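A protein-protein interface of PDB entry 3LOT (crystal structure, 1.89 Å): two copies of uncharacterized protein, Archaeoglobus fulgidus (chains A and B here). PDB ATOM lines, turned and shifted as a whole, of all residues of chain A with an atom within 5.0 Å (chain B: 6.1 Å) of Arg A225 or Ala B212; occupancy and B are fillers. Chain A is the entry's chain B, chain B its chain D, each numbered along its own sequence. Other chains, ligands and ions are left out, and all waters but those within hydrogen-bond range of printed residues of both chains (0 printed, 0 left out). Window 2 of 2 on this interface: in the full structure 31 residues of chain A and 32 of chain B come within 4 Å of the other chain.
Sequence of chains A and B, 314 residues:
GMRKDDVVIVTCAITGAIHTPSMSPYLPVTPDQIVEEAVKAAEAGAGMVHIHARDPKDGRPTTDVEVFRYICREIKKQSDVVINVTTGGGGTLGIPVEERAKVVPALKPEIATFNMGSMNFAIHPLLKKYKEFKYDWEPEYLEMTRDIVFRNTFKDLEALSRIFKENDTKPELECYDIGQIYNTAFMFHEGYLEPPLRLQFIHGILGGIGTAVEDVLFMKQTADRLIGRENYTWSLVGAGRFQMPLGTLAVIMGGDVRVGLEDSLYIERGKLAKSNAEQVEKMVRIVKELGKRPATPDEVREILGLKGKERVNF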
ATOM      1  N   ILE A 178     -24.979  28.357  28.147  1.00  0.00           N
ATOM      2  CA  ILE A 178     -25.907  28.818  27.091  1.00  0.00           C
ATOM      3  C   ILE A 178     -27.212  29.363  27.663  1.00  0.00           C
ATOM      4  O   ILE A 178     -27.708  30.437  27.236  1.00  0.00           O
ATOM      5  CB  ILE A 178     -26.173  27.694  26.095  1.00  0.00           C
ATOM      6  CG1 ILE A 178     -24.836  27.302  25.465  1.00  0.00           C
ATOM      7  CG2 ILE A 178     -27.167  28.123  25.019  1.00  0.00           C
ATOM      8  CD1 ILE A 178     -24.254  28.406  24.512  1.00  0.00           C
ATOM      9  N   TYR A 182     -29.442  32.895  27.101  1.00  0.00           N
ATOM     10  CA  TYR A 182     -30.881  32.973  27.012  1.00  0.00           C
ATOM     11  C   TYR A 182     -31.476  33.889  28.133  1.00  0.00           C
ATOM     12  O   TYR A 182     -32.360  34.703  27.866  1.00  0.00           O
ATOM     13  CB  TYR A 182     -31.488  31.564  27.031  1.00  0.00           C
ATOM     14  CG  TYR A 182     -31.571  30.922  25.654  1.00  0.00           C
ATOM     15  CD1 TYR A 182     -32.653  31.164  24.850  1.00  0.00           C
ATOM     16  CD2 TYR A 182     -30.593  30.027  25.184  1.00  0.00           C
ATOM     17  CE1 TYR A 182     -32.754  30.588  23.595  1.00  0.00           C
ATOM     18  CE2 TYR A 182     -30.696  29.421  23.929  1.00  0.00           C
ATOM     19  CZ  TYR A 182     -31.781  29.692  23.144  1.00  0.00           C
ATOM     20  OH  TYR A 182     -31.941  29.136  21.878  1.00  0.00           O
ATOM     21  N   PHE A 218     -20.064  28.379  20.229  1.00  0.00           N
ATOM     22  CA  PHE A 218     -21.497  28.257  20.431  1.00  0.00           C
ATOM     23  C   PHE A 218     -22.054  29.330  21.361  1.00  0.00           C
ATOM     24  O   PHE A 218     -23.129  29.909  21.092  1.00  0.00           O
ATOM     25  CB  PHE A 218     -21.871  26.850  20.924  1.00  0.00           C
ATOM     26  CG  PHE A 218     -23.333  26.544  20.753  1.00  0.00           C
ATOM     27  CD1 PHE A 218     -23.858  26.369  19.494  1.00  0.00           C
ATOM     28  CD2 PHE A 218     -24.182  26.501  21.847  1.00  0.00           C
ATOM     29  CE1 PHE A 218     -25.210  26.150  19.307  1.00  0.00           C
ATOM     30  CE2 PHE A 218     -25.559  26.280  21.672  1.00  0.00           C
ATOM     31  CZ  PHE A 218     -26.076  26.121  20.408  1.00  0.00           C
ATOM     32  N   GLN A 221     -22.029  32.514  19.042  1.00  0.00           N
ATOM     33  CA  GLN A 221     -23.114  32.356  18.072  1.00  0.00           C
ATOM     34  C   GLN A 221     -24.476  32.459  18.736  1.00  0.00           C
ATOM     35  O   GLN A 221     -25.406  32.963  18.139  1.00  0.00           O
ATOM     36  CB  GLN A 221     -23.036  30.996  17.404  1.00  0.00           C
ATOM     37  CG  GLN A 221     -21.821  30.838  16.481  1.00  0.00           C
ATOM     38  CD  GLN A 221     -21.693  29.437  15.973  1.00  0.00           C
ATOM     39  OE1 GLN A 221     -22.233  28.489  16.585  1.00  0.00           O
ATOM     40  NE2 GLN A 221     -20.963  29.266  14.877  1.00  0.00           N
ATOM     41  N   THR A 222     -24.605  31.970  19.960  1.00  0.00           N
ATOM     42  CA  THR A 222     -25.901  32.121  20.663  1.00  0.00           C
ATOM     43  C   THR A 222     -26.214  33.591  20.957  1.00  0.00           C
ATOM     44  O   THR A 222     -27.379  34.052  20.750  1.00  0.00           O
ATOM     45  CB  THR A 222     -25.980  31.284  21.909  1.00  0.00           C
ATOM     46  OG1 THR A 222     -25.838  29.914  21.549  1.00  0.00           O
ATOM     47  CG2 THR A 222     -27.314  31.505  22.611  1.00  0.00           C
ATOM     48  N   ALA A 223     -25.203  34.339  21.431  1.00  0.00           N
ATOM     49  CA  ALA A 223     -25.354  35.792  21.611  1.00  0.00           C
ATOM     50  C   ALA A 223     -25.672  36.489  20.306  1.00  0.00           C
ATOM     51  O   ALA A 223     -26.590  37.317  20.283  1.00  0.00           O
ATOM     52  CB  ALA A 223     -24.152  36.423  22.307  1.00  0.00           C
ATOM     53  N   ASP A 224     -24.975  36.176  19.207  1.00  0.00           N
ATOM     54  CA  ASP A 224     -25.320  36.815  17.940  1.00  0.00           C
ATOM     55  C   ASP A 224     -26.776  36.577  17.569  1.00  0.00           C
ATOM     56  O   ASP A 224     -27.461  37.520  17.184  1.00  0.00           O
ATOM     57  CB  ASP A 224     -24.476  36.338  16.748  1.00  0.00           C
ATOM     58  CG  ASP A 224     -23.015  36.790  16.798  1.00  0.00           C
ATOM     59  OD1 ASP A 224     -22.585  37.656  17.596  1.00  0.00           O
ATOM     60  OD2 ASP A 224     -22.273  36.213  16.007  1.00  0.00           O
ATOM     61  N   ARG A 225     -27.212  35.327  17.744  1.00  0.00           N
ATOM     62  CA  ARG A 225     -28.512  34.837  17.328  1.00  0.00           C
ATOM     63  C   ARG A 225     -29.700  35.375  18.183  1.00  0.00           C
ATOM     64  O   ARG A 225     -30.780  35.592  17.652  1.00  0.00           O
ATOM     65  CB  ARG A 225     -28.420  33.294  17.294  1.00  0.00           C
ATOM     66  CG  ARG A 225     -29.646  32.461  17.545  1.00  0.00           C
ATOM     67  CD  ARG A 225     -29.345  30.925  17.280  1.00  0.00           C
ATOM     68  NE  ARG A 225     -28.603  30.210  18.338  1.00  0.00           N
ATOM     69  CZ  ARG A 225     -29.140  29.686  19.453  1.00  0.00           C
ATOM     70  NH1 ARG A 225     -30.442  29.826  19.688  1.00  0.00           N
ATOM     71  NH2 ARG A 225     -28.365  29.011  20.339  1.00  0.00           N
ATOM     72  N   LEU A 226     -29.485  35.566  19.484  1.00  0.00           N
ATOM     73  CA  LEU A 226     -30.524  36.014  20.434  1.00  0.00           C
ATOM     74  C   LEU A 226     -30.486  37.537  20.671  1.00  0.00           C
ATOM     75  O   LEU A 226     -31.530  38.175  20.776  1.00  0.00           O
ATOM     76  CB  LEU A 226     -30.382  35.285  21.787  1.00  0.00           C
ATOM     77  CG  LEU A 226     -30.533  33.758  21.741  1.00  0.00           C
ATOM     78  CD1 LEU A 226     -30.299  33.108  23.156  1.00  0.00           C
ATOM     79  CD2 LEU A 226     -31.891  33.410  21.140  1.00  0.00           C
ATOM     80  N   ILE A 227     -29.284  38.108  20.744  1.00  0.00           N
ATOM     81  CA  ILE A 227     -29.076  39.516  21.094  1.00  0.00           C
ATOM     82  C   ILE A 227     -28.895  40.394  19.842  1.00  0.00           C
ATOM     83  O   ILE A 227     -29.399  41.515  19.807  1.00  0.00           O
ATOM     84  CB  ILE A 227     -27.895  39.659  22.092  1.00  0.00           C
ATOM     85  CG1 ILE A 227     -28.334  38.974  23.411  1.00  0.00           C
ATOM     86  CG2 ILE A 227     -27.511  41.108  22.304  1.00  0.00           C
ATOM     87  CD1 ILE A 227     -27.284  38.753  24.364  1.00  0.00           C
ATOM     88  N   GLY A 228     -28.213  39.851  18.830  1.00  0.00           N
ATOM     89  CA  GLY A 228     -27.871  40.593  17.615  1.00  0.00           C
ATOM     90  C   GLY A 228     -26.416  40.981  17.604  1.00  0.00           C
ATOM     91  O   GLY A 228     -25.916  41.526  18.577  1.00  0.00           O
ATOM     92  N   HIS B 203     -35.804  21.370  26.528  1.00  0.00           N
ATOM     93  CA  HIS B 203     -35.608  22.623  25.784  1.00  0.00           C
ATOM     94  C   HIS B 203     -36.768  23.557  26.003  1.00  0.00           C
ATOM     95  O   HIS B 203     -37.924  23.161  25.840  1.00  0.00           O
ATOM     96  CB  HIS B 203     -35.425  22.293  24.282  1.00  0.00           C
ATOM     97  CG  HIS B 203     -34.093  21.661  23.972  1.00  0.00           C
ATOM     98  ND1 HIS B 203     -33.021  22.378  23.474  1.00  0.00           N
ATOM     99  CD2 HIS B 203     -33.651  20.389  24.128  1.00  0.00           C
ATOM    100  CE1 HIS B 203     -31.987  21.571  23.318  1.00  0.00           C
ATOM    101  NE2 HIS B 203     -32.334  20.359  23.728  1.00  0.00           N
ATOM    102  N   ILE B 209     -31.649  26.137  28.452  1.00  0.00           N
ATOM    103  CA  ILE B 209     -31.428  26.300  27.015  1.00  0.00           C
ATOM    104  C   ILE B 209     -32.750  26.380  26.235  1.00  0.00           C
ATOM    105  O   ILE B 209     -33.750  25.816  26.658  1.00  0.00           O
ATOM    106  CB  ILE B 209     -30.539  25.165  26.478  1.00  0.00           C
ATOM    107  CG1 ILE B 209     -30.025  25.536  25.108  1.00  0.00           C
ATOM    108  CG2 ILE B 209     -31.280  23.790  26.457  1.00  0.00           C
ATOM    109  CD1 ILE B 209     -28.762  24.745  24.633  1.00  0.00           C
ATOM    110  N   GLY B 210     -32.741  27.127  25.121  1.00  0.00           N
ATOM    111  CA  GLY B 210     -33.901  27.334  24.277  1.00  0.00           C
ATOM    112  C   GLY B 210     -34.267  26.195  23.347  1.00  0.00           C
ATOM    113  O   GLY B 210     -33.841  25.056  23.516  1.00  0.00           O
ATOM    114  N   THR B 211     -35.076  26.525  22.373  1.00  0.00           N
ATOM    115  CA  THR B 211     -35.666  25.546  21.484  1.00  0.00           C
ATOM    116  C   THR B 211     -35.173  25.607  20.039  1.00  0.00           C
ATOM    117  O   THR B 211     -35.855  25.048  19.157  1.00  0.00           O
ATOM    118  CB  THR B 211     -37.189  25.745  21.439  1.00  0.00           C
ATOM    119  OG1 THR B 211     -37.422  27.115  21.188  1.00  0.00           O
ATOM    120  CG2 THR B 211     -37.865  25.367  22.758  1.00  0.00           C
ATOM    121  N   ALA B 212     -34.034  26.276  19.766  1.00  0.00           N
ATOM    122  CA  ALA B 212     -33.461  26.248  18.409  1.00  0.00           C
ATOM    123  C   ALA B 212     -32.999  24.833  18.051  1.00  0.00           C
ATOM    124  O   ALA B 212     -32.559  24.066  18.924  1.00  0.00           O
ATOM    125  CB  ALA B 212     -32.292  27.227  18.260  1.00  0.00           C
ATOM    126  N   VAL B 213     -33.089  24.512  16.761  1.00  0.00           N
ATOM    127  CA  VAL B 213     -32.479  23.321  16.210  1.00  0.00           C
ATOM    128  C   VAL B 213     -30.999  23.277  16.611  1.00  0.00           C
ATOM    129  O   VAL B 213     -30.517  22.240  17.012  1.00  0.00           O
ATOM    130  CB  VAL B 213     -32.667  23.280  14.666  1.00  0.00           C
ATOM    131  CG1 VAL B 213     -31.839  22.168  14.002  1.00  0.00           C
ATOM    132  CG2 VAL B 213     -34.177  23.082  14.375  1.00  0.00           C
ATOM    133  N   GLU B 214     -30.314  24.432  16.531  1.00  0.00           N
ATOM    134  CA  GLU B 214     -28.935  24.582  17.031  1.00  0.00           C
ATOM    135  C   GLU B 214     -28.713  24.061  18.463  1.00  0.00           C
ATOM    136  O   GLU B 214     -27.729  23.388  18.725  1.00  0.00           O
ATOM    137  CB  GLU B 214     -28.501  26.050  17.003  1.00  0.00           C
ATOM    138  CG  GLU B 214     -28.195  26.576  15.665  1.00  0.00           C
ATOM    139  CD  GLU B 214     -29.427  27.045  14.878  1.00  0.00           C
ATOM    140  OE1 GLU B 214     -30.611  26.720  15.265  1.00  0.00           O
ATOM    141  OE2 GLU B 214     -29.184  27.734  13.865  1.00  0.00           O
ATOM    142  N   ASP B 215     -29.624  24.408  19.381  1.00  0.00           N
ATOM    143  CA  ASP B 215     -29.533  23.997  20.775  1.00  0.00           C
ATOM    144  C   ASP B 215     -29.663  22.493  20.938  1.00  0.00           C
ATOM    145  O   ASP B 215     -28.937  21.867  21.711  1.00  0.00           O
ATOM    146  CB  ASP B 215     -30.642  24.637  21.622  1.00  0.00           C
ATOM    147  CG  ASP B 215     -30.583  26.161  21.677  1.00  0.00           C
ATOM    148  OD1 ASP B 215     -29.487  26.794  21.647  1.00  0.00           O
ATOM    149  OD2 ASP B 215     -31.695  26.742  21.749  1.00  0.00           O
ATOM    150  N   VAL B 216     -30.620  21.894  20.230  1.00  0.00           N
ATOM    151  CA  VAL B 216     -30.799  20.451  20.298  1.00  0.00           C
ATOM    152  C   VAL B 216     -29.526  19.744  19.790  1.00  0.00           C
ATOM    153  O   VAL B 216     -28.956  18.890  20.471  1.00  0.00           O
ATOM    154  CB  VAL B 216     -32.060  20.004  19.528  1.00  0.00           C
ATOM    155  CG1 VAL B 216     -32.130  18.471  19.518  1.00  0.00           C
ATOM    156  CG2 VAL B 216     -33.297  20.658  20.163  1.00  0.00           C
ATOM    157  N   LEU B 217     -29.037  20.164  18.635  1.00  0.00           N
ATOM    158  CA  LEU B 217     -27.864  19.507  18.061  1.00  0.00           C
ATOM    159  C   LEU B 217     -26.660  19.618  18.978  1.00  0.00           C
ATOM    160  O   LEU B 217     -25.937  18.614  19.198  1.00  0.00           O
ATOM    161  CB  LEU B 217     -27.551  20.040  16.675  1.00  0.00           C
ATOM    162  CG  LEU B 217     -26.471  19.242  15.933  1.00  0.00           C
ATOM    163  CD1 LEU B 217     -26.892  17.744  15.644  1.00  0.00           C
ATOM    164  CD2 LEU B 217     -26.146  19.996  14.658  1.00  0.00           C
ATOM    165  N   LEU B 246     -39.521  19.639  17.615  1.00  0.00           N
ATOM    166  CA  LEU B 246     -38.265  19.194  18.207  1.00  0.00           C
ATOM    167  C   LEU B 246     -38.317  17.696  18.540  1.00  0.00           C
ATOM    168  O   LEU B 246     -37.317  16.989  18.430  1.00  0.00           O
ATOM    169  CB  LEU B 246     -37.906  20.038  19.432  1.00  0.00           C
ATOM    170  CG  LEU B 246     -37.786  21.523  19.169  1.00  0.00           C
ATOM    171  CD1 LEU B 246     -37.200  22.239  20.388  1.00  0.00           C
ATOM    172  CD2 LEU B 246     -36.897  21.745  17.953  1.00  0.00           C
ATOM    173  N   LEU B 249     -37.426  16.196  15.242  1.00  0.00           N
ATOM    174  CA  LEU B 249     -35.981  16.359  15.138  1.00  0.00           C
ATOM    175  C   LEU B 249     -35.224  15.237  15.891  1.00  0.00           C
ATOM    176  O   LEU B 249     -34.325  14.582  15.334  1.00  0.00           O
ATOM    177  CB  LEU B 249     -35.563  17.729  15.675  1.00  0.00           C
ATOM    178  CG  LEU B 249     -34.082  18.075  15.709  1.00  0.00           C
ATOM    179  CD1 LEU B 249     -33.463  18.027  14.240  1.00  0.00           C
ATOM    180  CD2 LEU B 249     -33.888  19.478  16.362  1.00  0.00           C
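No position is printed for both chains.
Of the 7 pairs that touch across the chains among the printed residues, none has its exchanged pair printed and touching as well.
N of Ala B212 is in hydrogen-bond range of OD2 of Asp B215 (3.1 Å).
The backbone carbonyl oxygen (O) of Phe A218 lies within hydrogen-bond range of the side-chain hydroxyl (OG1) of Thr A222, at 2.7 Å.
A ring nitrogen (ND1) of His B203 is in hydrogen-bond range of the backbone carbonyl oxygen (O) of Gly B210 (2.8 Å).
NH1 of Arg A225 is in hydrogen-bond range of OH of Tyr A182, 2.7 Å away.
The side-chain hydroxyl of Thr A222 sits at hydrogen-bond distance from the guanidinium group of Arg A225.
The backbone NH (N) of Thr B211 sits at hydrogen-bond distance from the side-chain carboxylate (OD2) of Asp B215, 3.4 Å away.
Of the printed residues of chain B, Ile A178 touches Ile B209.
Of the printed residues of chain B, Tyr A182 touches Gly B210 and Asp B215.
Printed residues of chain B within 4 Å of Phe A218: Glu B214 (3.6 Å) and Asp B215 (3.7 Å).
Gln A221 touches none of the printed residues of chain B.
Of the printed residues of chain B, Arg A225 touches Ala B212 and Asp B215.
Of the printed residues of chain A, Gly B210 touches Tyr A182.
Of the printed residues of chain A, Glu B214 touches Phe A218.
Leu B246 touches none of the printed residues of chain A.
The nearest printed residue of chain B that does not touch Arg A225 is Glu B214 (4.4 Å).
The nearest printed residue of chain A that does not touch Ala B212 is Tyr A182 (4.1 Å).
The nearest printed residue of chain A that does not touch Gly B210 is Ile A178 (5.7 Å).
Printed residues of chain A that touch a printed residue of chain B: Ile A178, Tyr A182, Phe A218 and Arg A225.
Hydrophobic or aromatic side chains of chain A within 4 Å of the printed part of chain B: Ile A178, Tyr A182 and Phe A218.
Of the 12 printed residues of chain B, 5 touch a printed residue of chain A.
Printed residues of chain B that touch a printed residue of chain A: Ile B209, Gly B210, Ala B212, Glu B214 and Asp B215.
Hydrophobic or aromatic side chains of chain B within 4 Å of the printed part of chain A: Ile B209 and Ala B212.
Among the printed residues, Asp or Glu carboxylates within 4 Å of a Lys or Arg side-chain nitrogen of the other chain: Arg A225 with Asp B215.
The side-chain carboxylate (OD1) of Asp B215 lies within salt-bridge range of the guanidinium group (NH2) of Arg A225 (2.8 Å).
The side-chain hydroxyl (OH) of Tyr A182 sits at hydrogen-bond distance from the side-chain carboxylate (OD2) of Asp B215 (2.4 Å).
CD1 of Ile B209 touches CG2 of Ile A178 (3.8 Å).
Gly B210 touches Tyr A182.
O of Glu B214 touches CZ of Phe A218, 3.6 Å away.
Phe A218 touches Asp B215.
Arg A225 touches Ala B212.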
